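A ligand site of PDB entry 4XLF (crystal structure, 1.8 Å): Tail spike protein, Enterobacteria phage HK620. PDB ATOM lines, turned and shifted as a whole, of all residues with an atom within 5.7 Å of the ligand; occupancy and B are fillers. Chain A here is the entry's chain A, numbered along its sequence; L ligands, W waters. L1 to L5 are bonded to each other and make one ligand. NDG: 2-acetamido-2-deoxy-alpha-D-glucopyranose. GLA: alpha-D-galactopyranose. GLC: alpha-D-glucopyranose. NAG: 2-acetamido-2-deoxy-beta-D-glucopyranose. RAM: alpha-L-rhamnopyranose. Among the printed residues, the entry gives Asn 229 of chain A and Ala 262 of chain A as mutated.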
ATOM      1  N   GLY A 101      25.215  -9.005  21.645  1.00  0.00           N
ATOM      2  CA  GLY A 101      24.882  -8.079  22.727  1.00  0.00           C
ATOM      3  C   GLY A 101      23.822  -7.048  22.327  1.00  0.00           C
ATOM      4  O   GLY A 101      23.288  -6.350  23.193  1.00  0.00           O
ATOM      5  N   HIS A 102      23.515  -6.933  21.045  1.00  0.00           N
ATOM      6  CA  HIS A 102      22.548  -5.999  20.536  1.00  0.00           C
ATOM      7  C   HIS A 102      21.363  -6.716  19.913  1.00  0.00           C
ATOM      8  O   HIS A 102      20.613  -6.113  19.170  1.00  0.00           O
ATOM      9  CB  HIS A 102      23.188  -5.115  19.489  1.00  0.00           C
ATOM     10  CG  HIS A 102      24.459  -4.473  19.930  1.00  0.00           C
ATOM     11  ND1 HIS A 102      24.501  -3.204  20.434  1.00  0.00           N
ATOM     12  CD2 HIS A 102      25.724  -4.897  19.873  1.00  0.00           C
ATOM     13  CE1 HIS A 102      25.748  -2.847  20.650  1.00  0.00           C
ATOM     14  NE2 HIS A 102      26.522  -3.880  20.346  1.00  0.00           N
ATOM     15  N   SER A 103      21.165  -7.984  20.292  1.00  0.00           N
ATOM     16  CA  SER A 103      20.071  -8.815  19.658  1.00  0.00           C
ATOM     17  C   SER A 103      20.156  -8.738  18.146  1.00  0.00           C
ATOM     18  O   SER A 103      19.146  -8.801  17.478  1.00  0.00           O
ATOM     19  CB  SER A 103      18.708  -8.381  20.121  1.00  0.00           C
ATOM     20  OG  SER A 103      18.700  -8.245  21.535  1.00  0.00           O
ATOM     21  N   GLN A 132      17.658  -6.533  16.367  1.00  0.00           N
ATOM     22  CA  GLN A 132      18.147  -5.380  15.607  1.00  0.00           C
ATOM     23  C   GLN A 132      18.672  -5.919  14.363  1.00  0.00           C
ATOM     24  O   GLN A 132      19.645  -6.709  14.355  1.00  0.00           O
ATOM     25  CB  GLN A 132      19.220  -4.648  16.366  1.00  0.00           C
ATOM     26  CG  GLN A 132      18.663  -3.993  17.638  1.00  0.00           C
ATOM     27  CD  GLN A 132      19.628  -2.967  18.237  1.00  0.00           C
ATOM     28  OE1 GLN A 132      20.001  -1.940  17.608  1.00  0.00           O
ATOM     29  NE2 GLN A 132      19.947  -3.161  19.497  1.00  0.00           N
ATOM     30  N   PHE A 137      27.903  -2.215  15.031  1.00  0.00           N
ATOM     31  CA  PHE A 137      28.826  -2.449  16.132  1.00  0.00           C
ATOM     32  C   PHE A 137      29.549  -3.795  15.906  1.00  0.00           C
ATOM     33  O   PHE A 137      28.976  -4.711  15.342  1.00  0.00           O
ATOM     34  CB  PHE A 137      28.074  -2.489  17.466  1.00  0.00           C
ATOM     35  CG  PHE A 137      27.421  -1.172  17.889  1.00  0.00           C
ATOM     36  CD1 PHE A 137      28.197  -0.085  18.302  1.00  0.00           C
ATOM     37  CD2 PHE A 137      26.069  -1.088  17.960  1.00  0.00           C
ATOM     38  CE1 PHE A 137      27.546   1.086  18.730  1.00  0.00           C
ATOM     39  CE2 PHE A 137      25.407   0.016  18.416  1.00  0.00           C
ATOM     40  CZ  PHE A 137      26.165   1.114  18.819  1.00  0.00           C
ATOM     41  N   PRO A 142      29.241  -1.085  23.230  1.00  0.00           N
ATOM     42  CA  PRO A 142      29.507  -0.063  22.213  1.00  0.00           C
ATOM     43  C   PRO A 142      30.757   0.753  22.491  1.00  0.00           C
ATOM     44  O   PRO A 142      31.472   1.184  21.543  1.00  0.00           O
ATOM     45  CB  PRO A 142      28.233   0.798  22.206  1.00  0.00           C
ATOM     46  CG  PRO A 142      27.425   0.407  23.373  1.00  0.00           C
ATOM     47  CD  PRO A 142      27.898  -0.969  23.813  1.00  0.00           C
ATOM     48  N   LEU A 172      14.018  -4.064  23.127  1.00  0.00           N
ATOM     49  CA  LEU A 172      14.370  -3.083  22.048  1.00  0.00           C
ATOM     50  C   LEU A 172      14.332  -3.784  20.675  1.00  0.00           C
ATOM     51  O   LEU A 172      14.707  -4.974  20.511  1.00  0.00           O
ATOM     52  CB  LEU A 172      15.761  -2.429  22.262  1.00  0.00           C
ATOM     53  CG  LEU A 172      16.016  -1.760  23.627  1.00  0.00           C
ATOM     54  CD1 LEU A 172      17.508  -1.555  23.926  1.00  0.00           C
ATOM     55  CD2 LEU A 172      15.247  -0.489  23.756  1.00  0.00           C
ATOM     56  N   ASN A 174      15.066  -2.684  16.389  1.00  0.00           N
ATOM     57  CA  ASN A 174      15.668  -1.706  15.452  1.00  0.00           C
ATOM     58  C   ASN A 174      15.744  -2.390  14.086  1.00  0.00           C
ATOM     59  O   ASN A 174      15.859  -3.609  14.013  1.00  0.00           O
ATOM     60  CB  ASN A 174      17.065  -1.296  15.952  1.00  0.00           C
ATOM     61  CG  ASN A 174      17.635  -0.022  15.293  1.00  0.00           C
ATOM     62  OD1 ASN A 174      17.006   0.706  14.492  1.00  0.00           O
ATOM     63  ND2 ASN A 174      18.858   0.311  15.718  1.00  0.00           N
ATOM     64  N   THR A 197      11.290  -0.095  18.199  1.00  0.00           N
ATOM     65  CA  THR A 197      11.642   1.015  18.983  1.00  0.00           C
ATOM     66  C   THR A 197      12.138   2.156  18.022  1.00  0.00           C
ATOM     67  O   THR A 197      11.792   3.343  18.168  1.00  0.00           O
ATOM     68  CB  THR A 197      12.797   0.660  19.914  1.00  0.00           C
ATOM     69  OG1 THR A 197      12.485  -0.497  20.722  1.00  0.00           O
ATOM     70  CG2 THR A 197      13.120   1.872  20.754  1.00  0.00           C
ATOM     71  N   TRP A 198      12.961   1.760  17.089  1.00  0.00           N
ATOM     72  CA  TRP A 198      13.527   2.645  16.009  1.00  0.00           C
ATOM     73  C   TRP A 198      13.528   1.831  14.698  1.00  0.00           C
ATOM     74  O   TRP A 198      13.574   0.559  14.741  1.00  0.00           O
ATOM     75  CB  TRP A 198      14.965   3.037  16.277  1.00  0.00           C
ATOM     76  CG  TRP A 198      15.313   3.465  17.625  1.00  0.00           C
ATOM     77  CD1 TRP A 198      15.073   4.665  18.187  1.00  0.00           C
ATOM     78  CD2 TRP A 198      16.002   2.661  18.613  1.00  0.00           C
ATOM     79  NE1 TRP A 198      15.605   4.683  19.473  1.00  0.00           N
ATOM     80  CE2 TRP A 198      16.112   3.446  19.767  1.00  0.00           C
ATOM     81  CE3 TRP A 198      16.494   1.356  18.616  1.00  0.00           C
ATOM     82  CZ2 TRP A 198      16.733   2.956  20.948  1.00  0.00           C
ATOM     83  CZ3 TRP A 198      17.058   0.851  19.783  1.00  0.00           C
ATOM     84  CH2 TRP A 198      17.201   1.684  20.916  1.00  0.00           C
ATOM     85  N   THR A 201      19.071   3.813  13.451  1.00  0.00           N
ATOM     86  CA  THR A 201      19.847   4.687  14.290  1.00  0.00           C
ATOM     87  C   THR A 201      21.237   4.966  13.741  1.00  0.00           C
ATOM     88  O   THR A 201      21.835   4.091  13.096  1.00  0.00           O
ATOM     89  CB  THR A 201      20.073   4.098  15.686  1.00  0.00           C
ATOM     90  OG1 THR A 201      20.890   2.925  15.609  1.00  0.00           O
ATOM     91  CG2 THR A 201      18.743   3.800  16.338  1.00  0.00           C
ATOM     92  N   LEU A 202      21.668   6.199  13.917  1.00  0.00           N
ATOM     93  CA  LEU A 202      22.879   6.673  13.320  1.00  0.00           C
ATOM     94  C   LEU A 202      23.784   7.053  14.466  1.00  0.00           C
ATOM     95  O   LEU A 202      23.380   7.825  15.356  1.00  0.00           O
ATOM     96  CB  LEU A 202      22.644   7.909  12.480  1.00  0.00           C
ATOM     97  CG  LEU A 202      21.561   7.830  11.427  1.00  0.00           C
ATOM     98  CD1 LEU A 202      21.413   9.171  10.703  1.00  0.00           C
ATOM     99  CD2 LEU A 202      21.778   6.679  10.462  1.00  0.00           C
ATOM    100  N   GLY A 203      24.967   6.517  14.448  1.00  0.00           N
ATOM    101  CA  GLY A 203      25.977   6.944  15.446  1.00  0.00           C
ATOM    102  C   GLY A 203      25.758   6.326  16.795  1.00  0.00           C
ATOM    103  O   GLY A 203      24.792   5.604  17.024  1.00  0.00           O
ATOM    104  N   TRP A 204      26.656   6.643  17.716  1.00  0.00           N
ATOM    105  CA  TRP A 204      26.596   6.169  19.092  1.00  0.00           C
ATOM    106  C   TRP A 204      27.213   7.202  19.987  1.00  0.00           C
ATOM    107  O   TRP A 204      28.434   7.407  19.952  1.00  0.00           O
ATOM    108  CB  TRP A 204      27.231   4.789  19.319  1.00  0.00           C
ATOM    109  CG  TRP A 204      27.159   4.388  20.751  1.00  0.00           C
ATOM    110  CD1 TRP A 204      26.046   3.999  21.418  1.00  0.00           C
ATOM    111  CD2 TRP A 204      28.212   4.483  21.708  1.00  0.00           C
ATOM    112  NE1 TRP A 204      26.336   3.802  22.753  1.00  0.00           N
ATOM    113  CE2 TRP A 204      27.662   4.083  22.968  1.00  0.00           C
ATOM    114  CE3 TRP A 204      29.557   4.844  21.649  1.00  0.00           C
ATOM    115  CZ2 TRP A 204      28.409   4.037  24.102  1.00  0.00           C
ATOM    116  CZ3 TRP A 204      30.315   4.791  22.782  1.00  0.00           C
ATOM    117  CH2 TRP A 204      29.743   4.383  24.019  1.00  0.00           C
ATOM    118  N   ASN A 205      26.355   7.832  20.792  1.00  0.00           N
ATOM    119  CA  ASN A 205      26.739   8.809  21.804  1.00  0.00           C
ATOM    120  C   ASN A 205      27.766   9.791  21.332  1.00  0.00           C
ATOM    121  O   ASN A 205      28.764  10.011  21.988  1.00  0.00           O
ATOM    122  CB  ASN A 205      27.178   8.136  23.085  1.00  0.00           C
ATOM    123  CG  ASN A 205      26.067   7.432  23.808  1.00  0.00           C
ATOM    124  OD1 ASN A 205      24.896   7.432  23.378  1.00  0.00           O
ATOM    125  ND2 ASN A 205      26.440   6.734  24.884  1.00  0.00           N
ATOM    126  N   ASN A 229       7.922   2.994  23.530  1.00  0.00           N
ATOM    127  CA  ASN A 229       8.501   4.252  23.021  1.00  0.00           C
ATOM    128  C   ASN A 229       9.021   3.984  21.668  1.00  0.00           C
ATOM    129  O   ASN A 229       9.562   2.887  21.403  1.00  0.00           O
ATOM    130  CB  ASN A 229       9.636   4.709  23.940  1.00  0.00           C
ATOM    131  CG  ASN A 229       9.928   6.192  23.859  1.00  0.00           C
ATOM    132  OD1 ASN A 229       9.656   6.889  22.860  1.00  0.00           O
ATOM    133  ND2 ASN A 229      10.533   6.682  24.916  1.00  0.00           N
ATOM    134  N   HIS A 230       8.855   4.966  20.796  1.00  0.00           N
ATOM    135  CA  HIS A 230       9.322   4.838  19.432  1.00  0.00           C
ATOM    136  C   HIS A 230       9.822   6.138  18.854  1.00  0.00           C
ATOM    137  O   HIS A 230       9.159   7.149  19.055  1.00  0.00           O
ATOM    138  CB  HIS A 230       8.202   4.347  18.545  1.00  0.00           C
ATOM    139  CG  HIS A 230       8.577   4.268  17.089  1.00  0.00           C
ATOM    140  ND1 HIS A 230       8.929   3.087  16.459  1.00  0.00           N
ATOM    141  CD2 HIS A 230       8.593   5.223  16.129  1.00  0.00           C
ATOM    142  CE1 HIS A 230       9.151   3.329  15.189  1.00  0.00           C
ATOM    143  NE2 HIS A 230       8.947   4.613  14.962  1.00  0.00           N
ATOM    144  N   SER A 231      10.991   6.090  18.241  1.00  0.00           N
ATOM    145  CA  SER A 231      11.574   7.198  17.431  1.00  0.00           C
ATOM    146  C   SER A 231      12.094   6.582  16.125  1.00  0.00           C
ATOM    147  O   SER A 231      12.993   5.773  16.145  1.00  0.00           O
ATOM    148  CB  SER A 231      12.686   7.948  18.139  1.00  0.00           C
ATOM    149  OG  SER A 231      13.058   9.052  17.340  1.00  0.00           O
ATOM    150  N   TYR A 234      16.874   7.802  14.968  1.00  0.00           N
ATOM    151  CA  TYR A 234      17.615   8.468  16.018  1.00  0.00           C
ATOM    152  C   TYR A 234      19.019   8.884  15.536  1.00  0.00           C
ATOM    153  O   TYR A 234      19.798   8.038  15.108  1.00  0.00           O
ATOM    154  CB  TYR A 234      17.683   7.536  17.223  1.00  0.00           C
ATOM    155  CG  TYR A 234      17.949   8.074  18.618  1.00  0.00           C
ATOM    156  CD1 TYR A 234      19.198   8.537  19.000  1.00  0.00           C
ATOM    157  CD2 TYR A 234      16.968   8.011  19.604  1.00  0.00           C
ATOM    158  CE1 TYR A 234      19.435   8.985  20.316  1.00  0.00           C
ATOM    159  CE2 TYR A 234      17.228   8.447  20.895  1.00  0.00           C
ATOM    160  CZ  TYR A 234      18.450   8.904  21.265  1.00  0.00           C
ATOM    161  OH  TYR A 234      18.712   9.267  22.583  1.00  0.00           O
ATOM    162  N   ASN A 236      22.448  10.179  16.373  1.00  0.00           N
ATOM    163  CA  ASN A 236      23.326  10.285  17.519  1.00  0.00           C
ATOM    164  C   ASN A 236      24.796  10.456  17.119  1.00  0.00           C
ATOM    165  O   ASN A 236      25.696  10.073  17.826  1.00  0.00           O
ATOM    166  CB  ASN A 236      23.155   9.066  18.413  1.00  0.00           C
ATOM    167  CG  ASN A 236      23.392   9.378  19.898  1.00  0.00           C
ATOM    168  OD1 ASN A 236      23.708  10.484  20.255  1.00  0.00           O
ATOM    169  ND2 ASN A 236      23.269   8.343  20.728  1.00  0.00           N
ATOM    170  N   ALA A 262      14.741  11.919  16.133  1.00  0.00           N
ATOM    171  CA  ALA A 262      15.412  12.524  17.247  1.00  0.00           C
ATOM    172  C   ALA A 262      16.739  13.100  16.723  1.00  0.00           C
ATOM    173  O   ALA A 262      17.587  12.340  16.248  1.00  0.00           O
ATOM    174  CB  ALA A 262      15.712  11.511  18.345  1.00  0.00           C
ATOM    175  N   HIS A 264      20.111  14.515  18.035  1.00  0.00           N
ATOM    176  CA  HIS A 264      20.762  14.529  19.326  1.00  0.00           C
ATOM    177  C   HIS A 264      22.247  14.886  19.354  1.00  0.00           C
ATOM    178  O   HIS A 264      22.902  14.698  20.396  1.00  0.00           O
ATOM    179  CB  HIS A 264      20.568  13.156  20.018  1.00  0.00           C
ATOM    180  CG  HIS A 264      19.265  12.976  20.740  1.00  0.00           C
ATOM    181  ND1 HIS A 264      19.182  12.204  21.870  1.00  0.00           N
ATOM    182  CD2 HIS A 264      18.021  13.425  20.514  1.00  0.00           C
ATOM    183  CE1 HIS A 264      17.940  12.179  22.318  1.00  0.00           C
ATOM    184  NE2 HIS A 264      17.196  12.850  21.474  1.00  0.00           N
ATOM    185  N   TYR A 283      12.326  15.309  18.219  1.00  0.00           N
ATOM    186  CA  TYR A 283      13.096  15.776  19.394  1.00  0.00           C
ATOM    187  C   TYR A 283      14.423  16.464  18.930  1.00  0.00           C
ATOM    188  O   TYR A 283      15.126  15.970  18.070  1.00  0.00           O
ATOM    189  CB  TYR A 283      13.451  14.640  20.381  1.00  0.00           C
ATOM    190  CG  TYR A 283      12.262  14.142  21.152  1.00  0.00           C
ATOM    191  CD1 TYR A 283      11.894  14.753  22.352  1.00  0.00           C
ATOM    192  CD2 TYR A 283      11.483  13.070  20.710  1.00  0.00           C
ATOM    193  CE1 TYR A 283      10.800  14.302  23.083  1.00  0.00           C
ATOM    194  CE2 TYR A 283      10.431  12.636  21.439  1.00  0.00           C
ATOM    195  CZ  TYR A 283      10.083  13.242  22.618  1.00  0.00           C
ATOM    196  OH  TYR A 283       8.981  12.795  23.312  1.00  0.00           O
ATOM    197  N   VAL A 285      17.557  17.590  21.160  1.00  0.00           N
ATOM    198  CA  VAL A 285      17.875  17.404  22.584  1.00  0.00           C
ATOM    199  C   VAL A 285      19.354  17.149  22.682  1.00  0.00           C
ATOM    200  O   VAL A 285      19.918  16.428  21.834  1.00  0.00           O
ATOM    201  CB  VAL A 285      17.078  16.213  23.146  1.00  0.00           C
ATOM    202  CG1 VAL A 285      17.527  15.878  24.609  1.00  0.00           C
ATOM    203  CG2 VAL A 285      15.572  16.497  23.131  1.00  0.00           C
ATOM    204  N   HIS A 287      21.345  15.194  25.380  1.00  0.00           N
ATOM    205  CA  HIS A 287      21.477  14.379  26.593  1.00  0.00           C
ATOM    206  C   HIS A 287      22.950  14.366  27.064  1.00  0.00           C
ATOM    207  O   HIS A 287      23.875  13.930  26.305  1.00  0.00           O
ATOM    208  CB  HIS A 287      21.107  12.941  26.327  1.00  0.00           C
ATOM    209  CG  HIS A 287      19.644  12.663  26.209  1.00  0.00           C
ATOM    210  ND1 HIS A 287      18.671  13.263  26.962  1.00  0.00           N
ATOM    211  CD2 HIS A 287      18.983  11.773  25.417  1.00  0.00           C
ATOM    212  CE1 HIS A 287      17.486  12.779  26.646  1.00  0.00           C
ATOM    213  NE2 HIS A 287      17.640  11.912  25.661  1.00  0.00           N
ATOM    214  N   ALA A 289      24.135  12.315  28.923  1.00  0.00           N
ATOM    215  CA  ALA A 289      24.514  10.920  28.787  1.00  0.00           C
ATOM    216  C   ALA A 289      25.038  10.479  27.447  1.00  0.00           C
ATOM    217  O   ALA A 289      25.566   9.358  27.333  1.00  0.00           O
ATOM    218  CB  ALA A 289      23.303  10.043  29.152  1.00  0.00           C
ATOM    219  N   GLU A 290      24.839  11.287  26.406  1.00  0.00           N
ATOM    220  CA  GLU A 290      25.226  10.947  25.091  1.00  0.00           C
ATOM    221  C   GLU A 290      26.363  11.836  24.604  1.00  0.00           C
ATOM    222  O   GLU A 290      26.621  11.896  23.434  1.00  0.00           O
ATOM    223  CB  GLU A 290      23.986  11.072  24.148  1.00  0.00           C
ATOM    224  CG  GLU A 290      22.895  10.084  24.537  1.00  0.00           C
ATOM    225  CD  GLU A 290      21.709  10.114  23.610  1.00  0.00           C
ATOM    226  OE1 GLU A 290      21.441  11.187  23.010  1.00  0.00           O
ATOM    227  OE2 GLU A 290      21.022   9.100  23.487  1.00  0.00           O
ATOM    228  N   ASN A 361      13.981  13.440  31.133  1.00  0.00           N
ATOM    229  CA  ASN A 361      13.286  12.163  31.231  1.00  0.00           C
ATOM    230  C   ASN A 361      12.821  11.797  32.646  1.00  0.00           C
ATOM    231  O   ASN A 361      11.915  11.035  32.769  1.00  0.00           O
ATOM    232  CB  ASN A 361      14.106  10.997  30.623  1.00  0.00           C
ATOM    233  CG  ASN A 361      14.159  11.073  29.113  1.00  0.00           C
ATOM    234  OD1 ASN A 361      13.411  11.827  28.515  1.00  0.00           O
ATOM    235  ND2 ASN A 361      15.047  10.303  28.484  1.00  0.00           N
HETATM  236  C1  NDG L   1      12.398   9.849  22.978  1.00  0.00           C
HETATM  237  C2  NDG L   1      13.520   8.807  22.900  1.00  0.00           C
HETATM  238  C3  NDG L   1      14.318   8.807  24.212  1.00  0.00           C
HETATM  239  C4  NDG L   1      14.837  10.255  24.454  1.00  0.00           C
HETATM  240  C5  NDG L   1      13.711  11.351  24.382  1.00  0.00           C
HETATM  241  C6  NDG L   1      14.309  12.785  24.210  1.00  0.00           C
HETATM  242  C7  NDG L   1      13.410   6.681  21.684  1.00  0.00           C
HETATM  243  C8  NDG L   1      12.599   5.470  21.413  1.00  0.00           C
HETATM  244  O5  NDG L   1      12.883  11.145  23.235  1.00  0.00           O
HETATM  245  O3  NDG L   1      15.417   7.882  24.167  1.00  0.00           O
HETATM  246  O4  NDG L   1      15.530  10.396  25.693  1.00  0.00           O
HETATM  247  O6  NDG L   1      14.645  12.858  22.755  1.00  0.00           O
HETATM  248  O7  NDG L   1      14.531   6.863  21.143  1.00  0.00           O
HETATM  249  N2  NDG L   1      12.874   7.552  22.563  1.00  0.00           N
HETATM  250  O1  NDG L   1      11.510   9.480  23.978  1.00  0.00           O
HETATM  251  C1  GLA L   2      15.711   7.301  25.441  1.00  0.00           C
HETATM  252  C2  GLA L   2      17.177   6.867  25.324  1.00  0.00           C
HETATM  253  C3  GLA L   2      17.339   5.777  24.224  1.00  0.00           C
HETATM  254  C4  GLA L   2      16.358   4.643  24.429  1.00  0.00           C
HETATM  255  C5  GLA L   2      14.935   5.218  24.514  1.00  0.00           C
HETATM  256  C6  GLA L   2      13.845   4.202  24.800  1.00  0.00           C
HETATM  257  O2  GLA L   2      17.967   8.005  24.994  1.00  0.00           O
HETATM  258  O3  GLA L   2      18.683   5.318  24.314  1.00  0.00           O
HETATM  259  O4  GLA L   2      16.648   3.951  25.681  1.00  0.00           O
HETATM  260  O5  GLA L   2      14.870   6.195  25.582  1.00  0.00           O
HETATM  261  O6  GLA L   2      13.863   3.159  23.823  1.00  0.00           O
HETATM  262  C1  GLC L   3      16.718   2.526  25.511  1.00  0.00           C
HETATM  263  C2  GLC L   3      16.796   1.873  26.898  1.00  0.00           C
HETATM  264  C3  GLC L   3      18.142   2.181  27.598  1.00  0.00           C
HETATM  265  C4  GLC L   3      19.235   1.685  26.690  1.00  0.00           C
HETATM  266  C5  GLC L   3      19.133   2.424  25.327  1.00  0.00           C
HETATM  267  C6  GLC L   3      20.177   2.032  24.277  1.00  0.00           C
HETATM  268  O2  GLC L   3      15.736   2.383  27.690  1.00  0.00           O
HETATM  269  O3  GLC L   3      18.123   1.427  28.808  1.00  0.00           O
HETATM  270  O4  GLC L   3      20.461   1.959  27.298  1.00  0.00           O
HETATM  271  O5  GLC L   3      17.835   2.117  24.751  1.00  0.00           O
HETATM  272  O6  GLC L   3      20.099   0.588  24.102  1.00  0.00           O
HETATM  273  C1  NAG L   4      19.501   5.764  23.208  1.00  0.00           C
HETATM  274  C2  NAG L   4      20.937   5.615  23.753  1.00  0.00           C
HETATM  275  C3  NAG L   4      21.952   5.876  22.646  1.00  0.00           C
HETATM  276  C4  NAG L   4      21.618   5.236  21.302  1.00  0.00           C
HETATM  277  C5  NAG L   4      20.200   5.509  20.988  1.00  0.00           C
HETATM  278  C6  NAG L   4      19.729   4.795  19.777  1.00  0.00           C
HETATM  279  C7  NAG L   4      21.291   6.226  26.073  1.00  0.00           C
HETATM  280  C8  NAG L   4      21.300   7.314  27.098  1.00  0.00           C
HETATM  281  N2  NAG L   4      21.025   6.576  24.830  1.00  0.00           N
HETATM  282  O3  NAG L   4      23.201   5.406  23.117  1.00  0.00           O
HETATM  283  O4  NAG L   4      22.473   5.788  20.250  1.00  0.00           O
HETATM  284  O5  NAG L   4      19.380   5.024  22.007  1.00  0.00           O
HETATM  285  O6  NAG L   4      19.862   3.397  19.850  1.00  0.00           O
HETATM  286  O7  NAG L   4      21.556   5.060  26.393  1.00  0.00           O
HETATM  287  C1  RAM L   5      21.360   0.027  24.529  1.00  0.00           C
HETATM  288  C2  RAM L   5      21.224  -1.483  24.369  1.00  0.00           C
HETATM  289  C3  RAM L   5      21.253  -1.874  22.933  1.00  0.00           C
HETATM  290  C4  RAM L   5      22.434  -1.233  22.201  1.00  0.00           C
HETATM  291  C5  RAM L   5      22.374   0.253  22.400  1.00  0.00           C
HETATM  292  C6  RAM L   5      23.640   0.954  21.865  1.00  0.00           C
HETATM  293  O2  RAM L   5      22.336  -2.080  25.048  1.00  0.00           O
HETATM  294  O3  RAM L   5      21.399  -3.312  22.935  1.00  0.00           O
HETATM  295  O4  RAM L   5      22.358  -1.645  20.820  1.00  0.00           O
HETATM  296  O5  RAM L   5      22.461   0.534  23.811  1.00  0.00           O
HETATM  297  O   HOH W   1      18.943  -5.022  22.196  1.00  0.00           O
HETATM  298  O   HOH W   2       8.992  10.248  24.069  1.00  0.00           O
HETATM  299  O   HOH W   3      21.446   6.528  17.345  1.00  0.00           O
HETATM  300  O   HOH W   4      17.492  -0.996  29.449  1.00  0.00           O
HETATM  301  O   HOH W   5      21.587   2.190  18.082  1.00  0.00           O
HETATM  302  O   HOH W   6      16.302   1.545  30.646  1.00  0.00           O
HETATM  303  O   HOH W   7      24.555   5.097  26.488  1.00  0.00           O
HETATM  304  O   HOH W   8      11.819   1.592  24.316  1.00  0.00           O
HETATM  305  O   HOH W   9      21.946  -0.378  18.547  1.00  0.00           O
HETATM  306  O   HOH W  10      19.949   1.981  30.936  1.00  0.00           O
HETATM  307  O   HOH W  11      23.737   3.902  18.931  1.00  0.00           O
HETATM  308  O   HOH W  12      14.551  -0.488  27.730  1.00  0.00           O
HETATM  309  O   HOH W  13      21.102  -5.217  24.673  1.00  0.00           O
HETATM  310  O   HOH W  14      18.178   9.038  27.677  1.00  0.00           O
HETATM  311  O   HOH W  15      15.305   5.051  28.183  1.00  0.00           O
HETATM  312  O   HOH W  16      24.134   3.009  24.585  1.00  0.00           O
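Merely in contact with the ligand: Tyr 283 (3.1 Å), Leu 172 (3.4 Å), Thr 197 (3.4 Å), Trp 204 (3.5 Å), Gly 101 (3.6 Å), Ser 231 (3.6 Å), Thr 201 (3.7 Å), Val 285 (3.8 Å), His 230 (3.8 Å), Ala 289 (3.96 Å), Phe 137 (3.96 Å) and Gly 203 (3.98 Å).
Hydrophobic or aromatic side chains within 4 Å of the ligand: His 102, Phe 137, Leu 172, Trp 198, Trp 204, Tyr 234, His 264, Tyr 283, Val 285, His 287 and Ala 289.
Within 4 Å of the ligand: Gly 101, His 102, Gln 132, Phe 137, Leu 172, Thr 197, Trp 198, Thr 201, Gly 203, Trp 204, Asn 205, Asn 229, His 230, Ser 231, Tyr 234, Asn 236, His 264, Tyr 283, Val 285, His 287, Ala 289, Glu 290 and Asn 361.
The side-chain amide nitrogen of Gln 132 lies within hydrogen-bond range of the backbone carbonyl oxygen of His 102 (3.0 Å).
The backbone NH (N) of Asn 236 sits at hydrogen-bond distance from the backbone carbonyl oxygen (O) of Leu 202 (2.7 Å).
The side-chain hydroxyl of Tyr 234 sits close to a ring nitrogen (ND1) of His 264 (3.1 Å).
ND1 of His 264 sits at hydrogen-bond distance from OE1 of Glu 290.
O of Trp 198 lies close to OD1 of Asn 174 (3.4 Å).
The backbone NH of Gln 132 is in hydrogen-bond range of the backbone carbonyl oxygen of Ser 103 (2.9 Å).
The backbone NH of Ser 231 is in hydrogen-bond range of the backbone carbonyl oxygen of Thr 197.
ND1 of His 230 sits close to O of Thr 197 (3.3 Å).
Water W9 bridges O4 of RAM L5 (2.6 Å) and OE1 of Gln 132 (2.7 Å).
Water W5 bridges the side-chain hydroxyl of Thr 201 (2.7 Å) and an oxygen (O6) of NAG L4 (2.7 Å).
Water W14 bridges an oxygen (O2) of GLA L2 and the side-chain amide nitrogen of Asn 361.
Water W16 bridges O3 of NAG L4 (3.0 Å) and NE1 of Trp 204 (3.0 Å).
Water W7 lies within hydrogen-bond range of ND2 of Asn 205 (3.0 Å) and O7 of NAG L4 (3.0 Å).
Water W1 lies within hydrogen-bond range of an oxygen (O3) of RAM L5, the side-chain hydroxyl (OG) of Ser 103 and the side-chain amide nitrogen (NE2) of Gln 132.
NE2 of His 287 sits at hydrogen-bond distance from O4 of NDG L1 (2.6 Å).
OD1 of Asn 205 sits at hydrogen-bond distance from O3 of NAG L4 (2.7 Å).
An oxygen (O4) of RAM L5 is in hydrogen-bond range of a ring nitrogen (ND1) of His 102 (2.7 Å).
O4 of NAG L4 is in hydrogen-bond range of ND2 of Asn 236 (2.7 Å).
O2 of GLA L2 is in hydrogen-bond range of OH of Tyr 234.
The side-chain amide nitrogen of Asn 361 is in hydrogen-bond range of an oxygen (O4) of NDG L1 (2.8 Å).
An oxygen (O6) of NDG L1 lies within hydrogen-bond range of a ring nitrogen (NE2) of His 264 (2.9 Å).
A nitrogen (N2) of NAG L4 lies within hydrogen-bond range of the side-chain carboxylate (OE2) of Glu 290 (2.9 Å).
The indole nitrogen of Trp 198 is in hydrogen-bond range of an oxygen (O7) of NDG L1 (2.9 Å).
O1 of NDG L1 lies within hydrogen-bond range of ND2 of Asn 229 (3.1 Å).
The side-chain amide nitrogen (NE2) of Gln 132 sits at hydrogen-bond distance from an oxygen (O4) of RAM L5, 3.1 Å away.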
